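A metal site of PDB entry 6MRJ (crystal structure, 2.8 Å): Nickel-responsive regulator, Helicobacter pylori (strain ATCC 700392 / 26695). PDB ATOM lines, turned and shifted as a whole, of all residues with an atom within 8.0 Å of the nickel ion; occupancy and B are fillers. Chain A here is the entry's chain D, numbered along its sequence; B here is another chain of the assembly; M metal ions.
ND1 of His 99 sits close to OH of Tyr 72, 3.3 Å away. The backbone carbonyl oxygen (O) of Asp 103 lies within hydrogen-bond range of a ring nitrogen (ND1) of His 88 of chain B (2.8 Å). The backbone NH of His 99 is in hydrogen-bond range of the backbone carbonyl oxygen of Thr 97 of chain B, at 2.8 Å. The side-chain carboxylate of Glu 109 sits at hydrogen-bond distance from a ring nitrogen (ND1) of His 99 (3.0 Å). A ring nitrogen (NE2) of His 101 lies within hydrogen-bond range of the side-chain amide oxygen (OE1) of Gln 87 of chain B, 2.8 Å away. The backbone NH of Cys 107 lies within hydrogen-bond range of the backbone carbonyl oxygen of Tyr 72, at 2.9 Å. The backbone carbonyl oxygen (O) of Ile 100 is in hydrogen-bond range of the backbone NH (N) of Leu 108.
Merely in contact with the nickel ion: Ile 100 (3.9 Å) and Ile 84 of chain B (3.5 Å). The nearest printed residue that does not touch the nickel ion is Asn 106 (4.4 Å).
The nickel ion is bound by NE2 of His 99 (2.0 Å), ND1 of His 101 (2.0 Å), NE2 of His 88 of chain B (2.1 Å) and SG of Cys 107 (2.2 Å). The nickel ion has four donor atoms within binding distance.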
ATOM      1  N   TYR A  72     -16.275 -10.819   1.515  1.00  0.00           N
ATOM      2  CA  TYR A  72     -16.956 -12.000   2.040  1.00  0.00           C
ATOM      3  C   TYR A  72     -17.286 -13.033   0.971  1.00  0.00           C
ATOM      4  O   TYR A  72     -17.275 -12.723  -0.228  1.00  0.00           O
ATOM      5  CB  TYR A  72     -18.246 -11.602   2.802  1.00  0.00           C
ATOM      6  CG  TYR A  72     -19.326 -10.973   1.933  1.00  0.00           C
ATOM      7  CD1 TYR A  72     -20.301 -11.763   1.330  1.00  0.00           C
ATOM      8  CD2 TYR A  72     -19.400  -9.600   1.763  1.00  0.00           C
ATOM      9  CE1 TYR A  72     -21.279 -11.200   0.509  1.00  0.00           C
ATOM     10  CE2 TYR A  72     -20.395  -9.020   0.967  1.00  0.00           C
ATOM     11  CZ  TYR A  72     -21.321  -9.828   0.323  1.00  0.00           C
ATOM     12  OH  TYR A  72     -22.329  -9.289  -0.447  1.00  0.00           O
ATOM     13  N   ASP A  73     -17.599 -14.262   1.413  1.00  0.00           N
ATOM     14  CA  ASP A  73     -18.020 -15.343   0.526  1.00  0.00           C
ATOM     15  C   ASP A  73     -19.539 -15.373   0.554  1.00  0.00           C
ATOM     16  O   ASP A  73     -20.145 -15.618   1.597  1.00  0.00           O
ATOM     17  CB  ASP A  73     -17.451 -16.693   0.971  1.00  0.00           C
ATOM     18  CG  ASP A  73     -17.581 -17.816  -0.051  1.00  0.00           C
ATOM     19  OD1 ASP A  73     -18.411 -17.686  -0.986  1.00  0.00           O
ATOM     20  OD2 ASP A  73     -16.853 -18.829   0.077  1.00  0.00           O
ATOM     21  N   HIS A  74     -20.148 -15.111  -0.608  1.00  0.00           N
ATOM     22  CA  HIS A  74     -21.603 -15.099  -0.727  1.00  0.00           C
ATOM     23  C   HIS A  74     -22.207 -16.504  -0.524  1.00  0.00           C
ATOM     24  O   HIS A  74     -23.395 -16.614  -0.220  1.00  0.00           O
ATOM     25  CB  HIS A  74     -22.040 -14.451  -2.057  1.00  0.00           C
ATOM     26  CG  HIS A  74     -22.002 -15.384  -3.221  1.00  0.00           C
ATOM     27  ND1 HIS A  74     -20.807 -15.743  -3.825  1.00  0.00           N
ATOM     28  CD2 HIS A  74     -23.019 -16.027  -3.834  1.00  0.00           C
ATOM     29  CE1 HIS A  74     -21.143 -16.581  -4.796  1.00  0.00           C
ATOM     30  NE2 HIS A  74     -22.463 -16.774  -4.844  1.00  0.00           N
ATOM     31  N   ASN A  80     -25.664 -13.017   3.616  1.00  0.00           N
ATOM     32  CA  ASN A  80     -26.202 -11.837   2.967  1.00  0.00           C
ATOM     33  C   ASN A  80     -27.435 -11.355   3.704  1.00  0.00           C
ATOM     34  O   ASN A  80     -27.501 -10.180   4.067  1.00  0.00           O
ATOM     35  CB  ASN A  80     -26.446 -12.075   1.470  1.00  0.00           C
ATOM     36  CG  ASN A  80     -25.166 -11.960   0.669  1.00  0.00           C
ATOM     37  OD1 ASN A  80     -24.598 -12.960   0.216  1.00  0.00           O
ATOM     38  ND2 ASN A  80     -24.648 -10.734   0.529  1.00  0.00           N
ATOM     39  N   HIS A  99     -21.262  -3.071  -4.735  1.00  0.00           N
ATOM     40  CA  HIS A  99     -20.795  -4.457  -4.727  1.00  0.00           C
ATOM     41  C   HIS A  99     -20.079  -4.853  -6.006  1.00  0.00           C
ATOM     42  O   HIS A  99     -20.565  -4.581  -7.100  1.00  0.00           O
ATOM     43  CB  HIS A  99     -22.012  -5.366  -4.501  1.00  0.00           C
ATOM     44  CG  HIS A  99     -21.686  -6.808  -4.344  1.00  0.00           C
ATOM     45  ND1 HIS A  99     -21.857  -7.426  -3.130  1.00  0.00           N
ATOM     46  CD2 HIS A  99     -21.273  -7.704  -5.248  1.00  0.00           C
ATOM     47  CE1 HIS A  99     -21.536  -8.690  -3.341  1.00  0.00           C
ATOM     48  NE2 HIS A  99     -21.147  -8.905  -4.592  1.00  0.00           N
ATOM     49  N   ILE A 100     -18.962  -5.580  -5.840  1.00  0.00           N
ATOM     50  CA  ILE A 100     -18.133  -6.150  -6.913  1.00  0.00           C
ATOM     51  C   ILE A 100     -18.027  -7.659  -6.699  1.00  0.00           C
ATOM     52  O   ILE A 100     -17.598  -8.104  -5.632  1.00  0.00           O
ATOM     53  CB  ILE A 100     -16.764  -5.452  -7.035  1.00  0.00           C
ATOM     54  CG1 ILE A 100     -16.981  -4.041  -7.635  1.00  0.00           C
ATOM     55  CG2 ILE A 100     -15.761  -6.267  -7.874  1.00  0.00           C
ATOM     56  CD1 ILE A 100     -16.206  -3.133  -7.122  1.00  0.00           C
ATOM     57  N   HIS A 101     -18.470  -8.443  -7.712  1.00  0.00           N
ATOM     58  CA  HIS A 101     -18.390  -9.901  -7.668  1.00  0.00           C
ATOM     59  C   HIS A 101     -17.008 -10.240  -8.190  1.00  0.00           C
ATOM     60  O   HIS A 101     -16.766 -10.189  -9.407  1.00  0.00           O
ATOM     61  CB  HIS A 101     -19.466 -10.533  -8.555  1.00  0.00           C
ATOM     62  CG  HIS A 101     -20.839  -9.981  -8.333  1.00  0.00           C
ATOM     63  ND1 HIS A 101     -21.523 -10.207  -7.146  1.00  0.00           N
ATOM     64  CD2 HIS A 101     -21.624  -9.249  -9.147  1.00  0.00           C
ATOM     65  CE1 HIS A 101     -22.700  -9.615  -7.294  1.00  0.00           C
ATOM     66  NE2 HIS A 101     -22.798  -9.020  -8.477  1.00  0.00           N
ATOM     67  N   MET A 102     -16.058 -10.461  -7.266  1.00  0.00           N
ATOM     68  CA  MET A 102     -14.657 -10.714  -7.595  1.00  0.00           C
ATOM     69  C   MET A 102     -14.443 -12.047  -8.298  1.00  0.00           C
ATOM     70  O   MET A 102     -13.919 -12.075  -9.408  1.00  0.00           O
ATOM     71  CB  MET A 102     -13.788 -10.585  -6.360  1.00  0.00           C
ATOM     72  CG  MET A 102     -13.689  -9.167  -5.905  1.00  0.00           C
ATOM     73  SD  MET A 102     -12.676  -9.085  -4.415  1.00  0.00           S
ATOM     74  CE  MET A 102     -11.040  -9.378  -5.103  1.00  0.00           C
ATOM     75  N   ASP A 103     -14.851 -13.147  -7.645  1.00  0.00           N
ATOM     76  CA  ASP A 103     -14.786 -14.515  -8.162  1.00  0.00           C
ATOM     77  C   ASP A 103     -15.928 -15.304  -7.528  1.00  0.00           C
ATOM     78  O   ASP A 103     -16.775 -14.695  -6.884  1.00  0.00           O
ATOM     79  CB  ASP A 103     -13.400 -15.158  -7.931  1.00  0.00           C
ATOM     80  CG  ASP A 103     -12.906 -15.121  -6.503  1.00  0.00           C
ATOM     81  OD1 ASP A 103     -13.502 -15.833  -5.652  1.00  0.00           O
ATOM     82  OD2 ASP A 103     -11.893 -14.439  -6.242  1.00  0.00           O
ATOM     83  N   GLU A 104     -15.970 -16.625  -7.703  1.00  0.00           N
ATOM     84  CA  GLU A 104     -17.043 -17.452  -7.156  1.00  0.00           C
ATOM     85  C   GLU A 104     -17.135 -17.399  -5.621  1.00  0.00           C
ATOM     86  O   GLU A 104     -18.241 -17.452  -5.090  1.00  0.00           O
ATOM     87  CB  GLU A 104     -16.949 -18.904  -7.675  1.00  0.00           C
ATOM     88  CG  GLU A 104     -18.227 -19.728  -7.570  1.00  0.00           C
ATOM     89  CD  GLU A 104     -19.488 -19.158  -8.202  1.00  0.00           C
ATOM     90  OE1 GLU A 104     -19.463 -18.878  -9.419  1.00  0.00           O
ATOM     91  OE2 GLU A 104     -20.499 -19.003  -7.475  1.00  0.00           O
ATOM     92  N   HIS A 105     -16.012 -17.249  -4.914  1.00  0.00           N
ATOM     93  CA  HIS A 105     -16.049 -17.205  -3.446  1.00  0.00           C
ATOM     94  C   HIS A 105     -15.656 -15.845  -2.832  1.00  0.00           C
ATOM     95  O   HIS A 105     -15.385 -15.777  -1.625  1.00  0.00           O
ATOM     96  CB  HIS A 105     -15.197 -18.360  -2.863  1.00  0.00           C
ATOM     97  CG  HIS A 105     -15.761 -19.716  -3.151  1.00  0.00           C
ATOM     98  ND1 HIS A 105     -16.586 -20.374  -2.235  1.00  0.00           N
ATOM     99  CD2 HIS A 105     -15.652 -20.490  -4.259  1.00  0.00           C
ATOM    100  CE1 HIS A 105     -16.924 -21.521  -2.809  1.00  0.00           C
ATOM    101  NE2 HIS A 105     -16.402 -21.626  -4.031  1.00  0.00           N
ATOM    102  N   ASN A 106     -15.655 -14.758  -3.646  1.00  0.00           N
ATOM    103  CA  ASN A 106     -15.294 -13.434  -3.146  1.00  0.00           C
ATOM    104  C   ASN A 106     -16.186 -12.294  -3.666  1.00  0.00           C
ATOM    105  O   ASN A 106     -16.467 -12.209  -4.865  1.00  0.00           O
ATOM    106  CB  ASN A 106     -13.817 -13.136  -3.410  1.00  0.00           C
ATOM    107  CG  ASN A 106     -12.880 -13.990  -2.579  1.00  0.00           C
ATOM    108  OD1 ASN A 106     -12.651 -13.739  -1.391  1.00  0.00           O
ATOM    109  ND2 ASN A 106     -12.372 -15.057  -3.161  1.00  0.00           N
ATOM    110  N   CYS A 107     -16.594 -11.410  -2.733  1.00  0.00           N
ATOM    111  CA  CYS A 107     -17.412 -10.223  -2.967  1.00  0.00           C
ATOM    112  C   CYS A 107     -16.799  -9.026  -2.275  1.00  0.00           C
ATOM    113  O   CYS A 107     -16.531  -9.084  -1.080  1.00  0.00           O
ATOM    114  CB  CYS A 107     -18.841 -10.435  -2.473  1.00  0.00           C
ATOM    115  SG  CYS A 107     -19.836 -11.527  -3.505  1.00  0.00           S
ATOM    116  N   LEU A 108     -16.583  -7.931  -3.017  1.00  0.00           N
ATOM    117  CA  LEU A 108     -16.087  -6.670  -2.472  1.00  0.00           C
ATOM    118  C   LEU A 108     -17.298  -5.770  -2.284  1.00  0.00           C
ATOM    119  O   LEU A 108     -18.174  -5.750  -3.136  1.00  0.00           O
ATOM    120  CB  LEU A 108     -15.065  -6.025  -3.423  1.00  0.00           C
ATOM    121  CG  LEU A 108     -14.227  -4.794  -2.960  1.00  0.00           C
ATOM    122  CD1 LEU A 108     -14.886  -3.470  -3.280  1.00  0.00           C
ATOM    123  CD2 LEU A 108     -13.817  -4.872  -1.522  1.00  0.00           C
ATOM    124  N   GLU A 109     -17.374  -5.064  -1.162  1.00  0.00           N
ATOM    125  CA  GLU A 109     -18.505  -4.194  -0.895  1.00  0.00           C
ATOM    126  C   GLU A 109     -18.108  -2.961  -0.099  1.00  0.00           C
ATOM    127  O   GLU A 109     -17.441  -3.086   0.927  1.00  0.00           O
ATOM    128  CB  GLU A 109     -19.619  -4.974  -0.189  1.00  0.00           C
ATOM    129  CG  GLU A 109     -21.009  -4.424  -0.431  1.00  0.00           C
ATOM    130  CD  GLU A 109     -22.093  -5.327   0.119  1.00  0.00           C
ATOM    131  OE1 GLU A 109     -22.184  -6.491  -0.342  1.00  0.00           O
ATOM    132  OE2 GLU A 109     -22.857  -4.875   1.002  1.00  0.00           O
ATOM    133  N   MET B  83     -30.063 -13.686  -5.975  1.00  0.00           N
ATOM    134  CA  MET B  83     -29.675 -12.624  -6.913  1.00  0.00           C
ATOM    135  C   MET B  83     -28.164 -12.564  -7.125  1.00  0.00           C
ATOM    136  O   MET B  83     -27.725 -12.459  -8.267  1.00  0.00           O
ATOM    137  CB  MET B  83     -30.173 -11.281  -6.394  1.00  0.00           C
ATOM    138  CG  MET B  83     -31.592 -10.986  -6.783  1.00  0.00           C
ATOM    139  SD  MET B  83     -32.214  -9.462  -6.030  1.00  0.00           S
ATOM    140  CE  MET B  83     -31.636  -8.299  -7.179  1.00  0.00           C
ATOM    141  N   ILE B  84     -27.381 -12.626  -6.024  1.00  0.00           N
ATOM    142  CA  ILE B  84     -25.908 -12.585  -6.078  1.00  0.00           C
ATOM    143  C   ILE B  84     -25.380 -13.864  -6.751  1.00  0.00           C
ATOM    144  O   ILE B  84     -24.434 -13.783  -7.536  1.00  0.00           O
ATOM    145  CB  ILE B  84     -25.256 -12.257  -4.704  1.00  0.00           C
ATOM    146  CG1 ILE B  84     -25.773 -10.934  -4.153  1.00  0.00           C
ATOM    147  CG2 ILE B  84     -23.722 -12.168  -4.838  1.00  0.00           C
ATOM    148  CD1 ILE B  84     -25.823 -10.872  -2.724  1.00  0.00           C
ATOM    149  N   ASP B  85     -26.033 -15.021  -6.504  1.00  0.00           N
ATOM    150  CA  ASP B  85     -25.680 -16.313  -7.116  1.00  0.00           C
ATOM    151  C   ASP B  85     -25.810 -16.226  -8.642  1.00  0.00           C
ATOM    152  O   ASP B  85     -24.890 -16.630  -9.352  1.00  0.00           O
ATOM    153  CB  ASP B  85     -26.559 -17.459  -6.582  1.00  0.00           C
ATOM    154  CG  ASP B  85     -26.030 -18.217  -5.370  1.00  0.00           C
ATOM    155  OD1 ASP B  85     -24.789 -18.453  -5.301  1.00  0.00           O
ATOM    156  OD2 ASP B  85     -26.860 -18.654  -4.538  1.00  0.00           O
ATOM    157  N   GLN B  87     -25.816 -13.474 -10.530  1.00  0.00           N
ATOM    158  CA  GLN B  87     -24.801 -12.532 -10.994  1.00  0.00           C
ATOM    159  C   GLN B  87     -23.390 -13.116 -11.017  1.00  0.00           C
ATOM    160  O   GLN B  87     -22.649 -12.843 -11.964  1.00  0.00           O
ATOM    161  CB  GLN B  87     -24.847 -11.241 -10.179  1.00  0.00           C
ATOM    162  CG  GLN B  87     -26.094 -10.413 -10.462  1.00  0.00           C
ATOM    163  CD  GLN B  87     -26.251  -9.288  -9.488  1.00  0.00           C
ATOM    164  OE1 GLN B  87     -25.407  -8.398  -9.398  1.00  0.00           O
ATOM    165  NE2 GLN B  87     -27.335  -9.308  -8.717  1.00  0.00           N
ATOM    166  N   HIS B  88     -23.026 -13.928 -10.013  1.00  0.00           N
ATOM    167  CA  HIS B  88     -21.709 -14.573  -9.988  1.00  0.00           C
ATOM    168  C   HIS B  88     -21.595 -15.622 -11.072  1.00  0.00           C
ATOM    169  O   HIS B  88     -20.532 -15.748 -11.683  1.00  0.00           O
ATOM    170  CB  HIS B  88     -21.415 -15.200  -8.621  1.00  0.00           C
ATOM    171  CG  HIS B  88     -20.816 -14.241  -7.649  1.00  0.00           C
ATOM    172  ND1 HIS B  88     -19.503 -14.349  -7.246  1.00  0.00           N
ATOM    173  CD2 HIS B  88     -21.369 -13.182  -7.045  1.00  0.00           C
ATOM    174  CE1 HIS B  88     -19.314 -13.361  -6.399  1.00  0.00           C
ATOM    175  NE2 HIS B  88     -20.414 -12.637  -6.252  1.00  0.00           N
ATOM    176  N   VAL B  94     -21.457  -8.747 -15.378  1.00  0.00           N
ATOM    177  CA  VAL B  94     -21.937  -7.862 -14.318  1.00  0.00           C
ATOM    178  C   VAL B  94     -20.784  -6.992 -13.839  1.00  0.00           C
ATOM    179  O   VAL B  94     -19.843  -7.519 -13.227  1.00  0.00           O
ATOM    180  CB  VAL B  94     -22.621  -8.619 -13.154  1.00  0.00           C
ATOM    181  CG1 VAL B  94     -23.209  -7.647 -12.136  1.00  0.00           C
ATOM    182  CG2 VAL B  94     -23.701  -9.569 -13.648  1.00  0.00           C
ATOM    183  N   THR B  97     -22.916  -3.483  -8.702  1.00  0.00           N
ATOM    184  CA  THR B  97     -24.291  -3.277  -8.214  1.00  0.00           C
ATOM    185  C   THR B  97     -24.318  -2.243  -7.088  1.00  0.00           C
ATOM    186  O   THR B  97     -23.587  -2.377  -6.108  1.00  0.00           O
ATOM    187  CB  THR B  97     -24.933  -4.617  -7.813  1.00  0.00           C
ATOM    188  OG1 THR B  97     -24.967  -5.493  -8.937  1.00  0.00           O
ATOM    189  CG2 THR B  97     -26.322  -4.448  -7.276  1.00  0.00           C
HETATM  190 NI    NI M   1     -20.577 -10.669  -5.405  1.00  0.00          NI
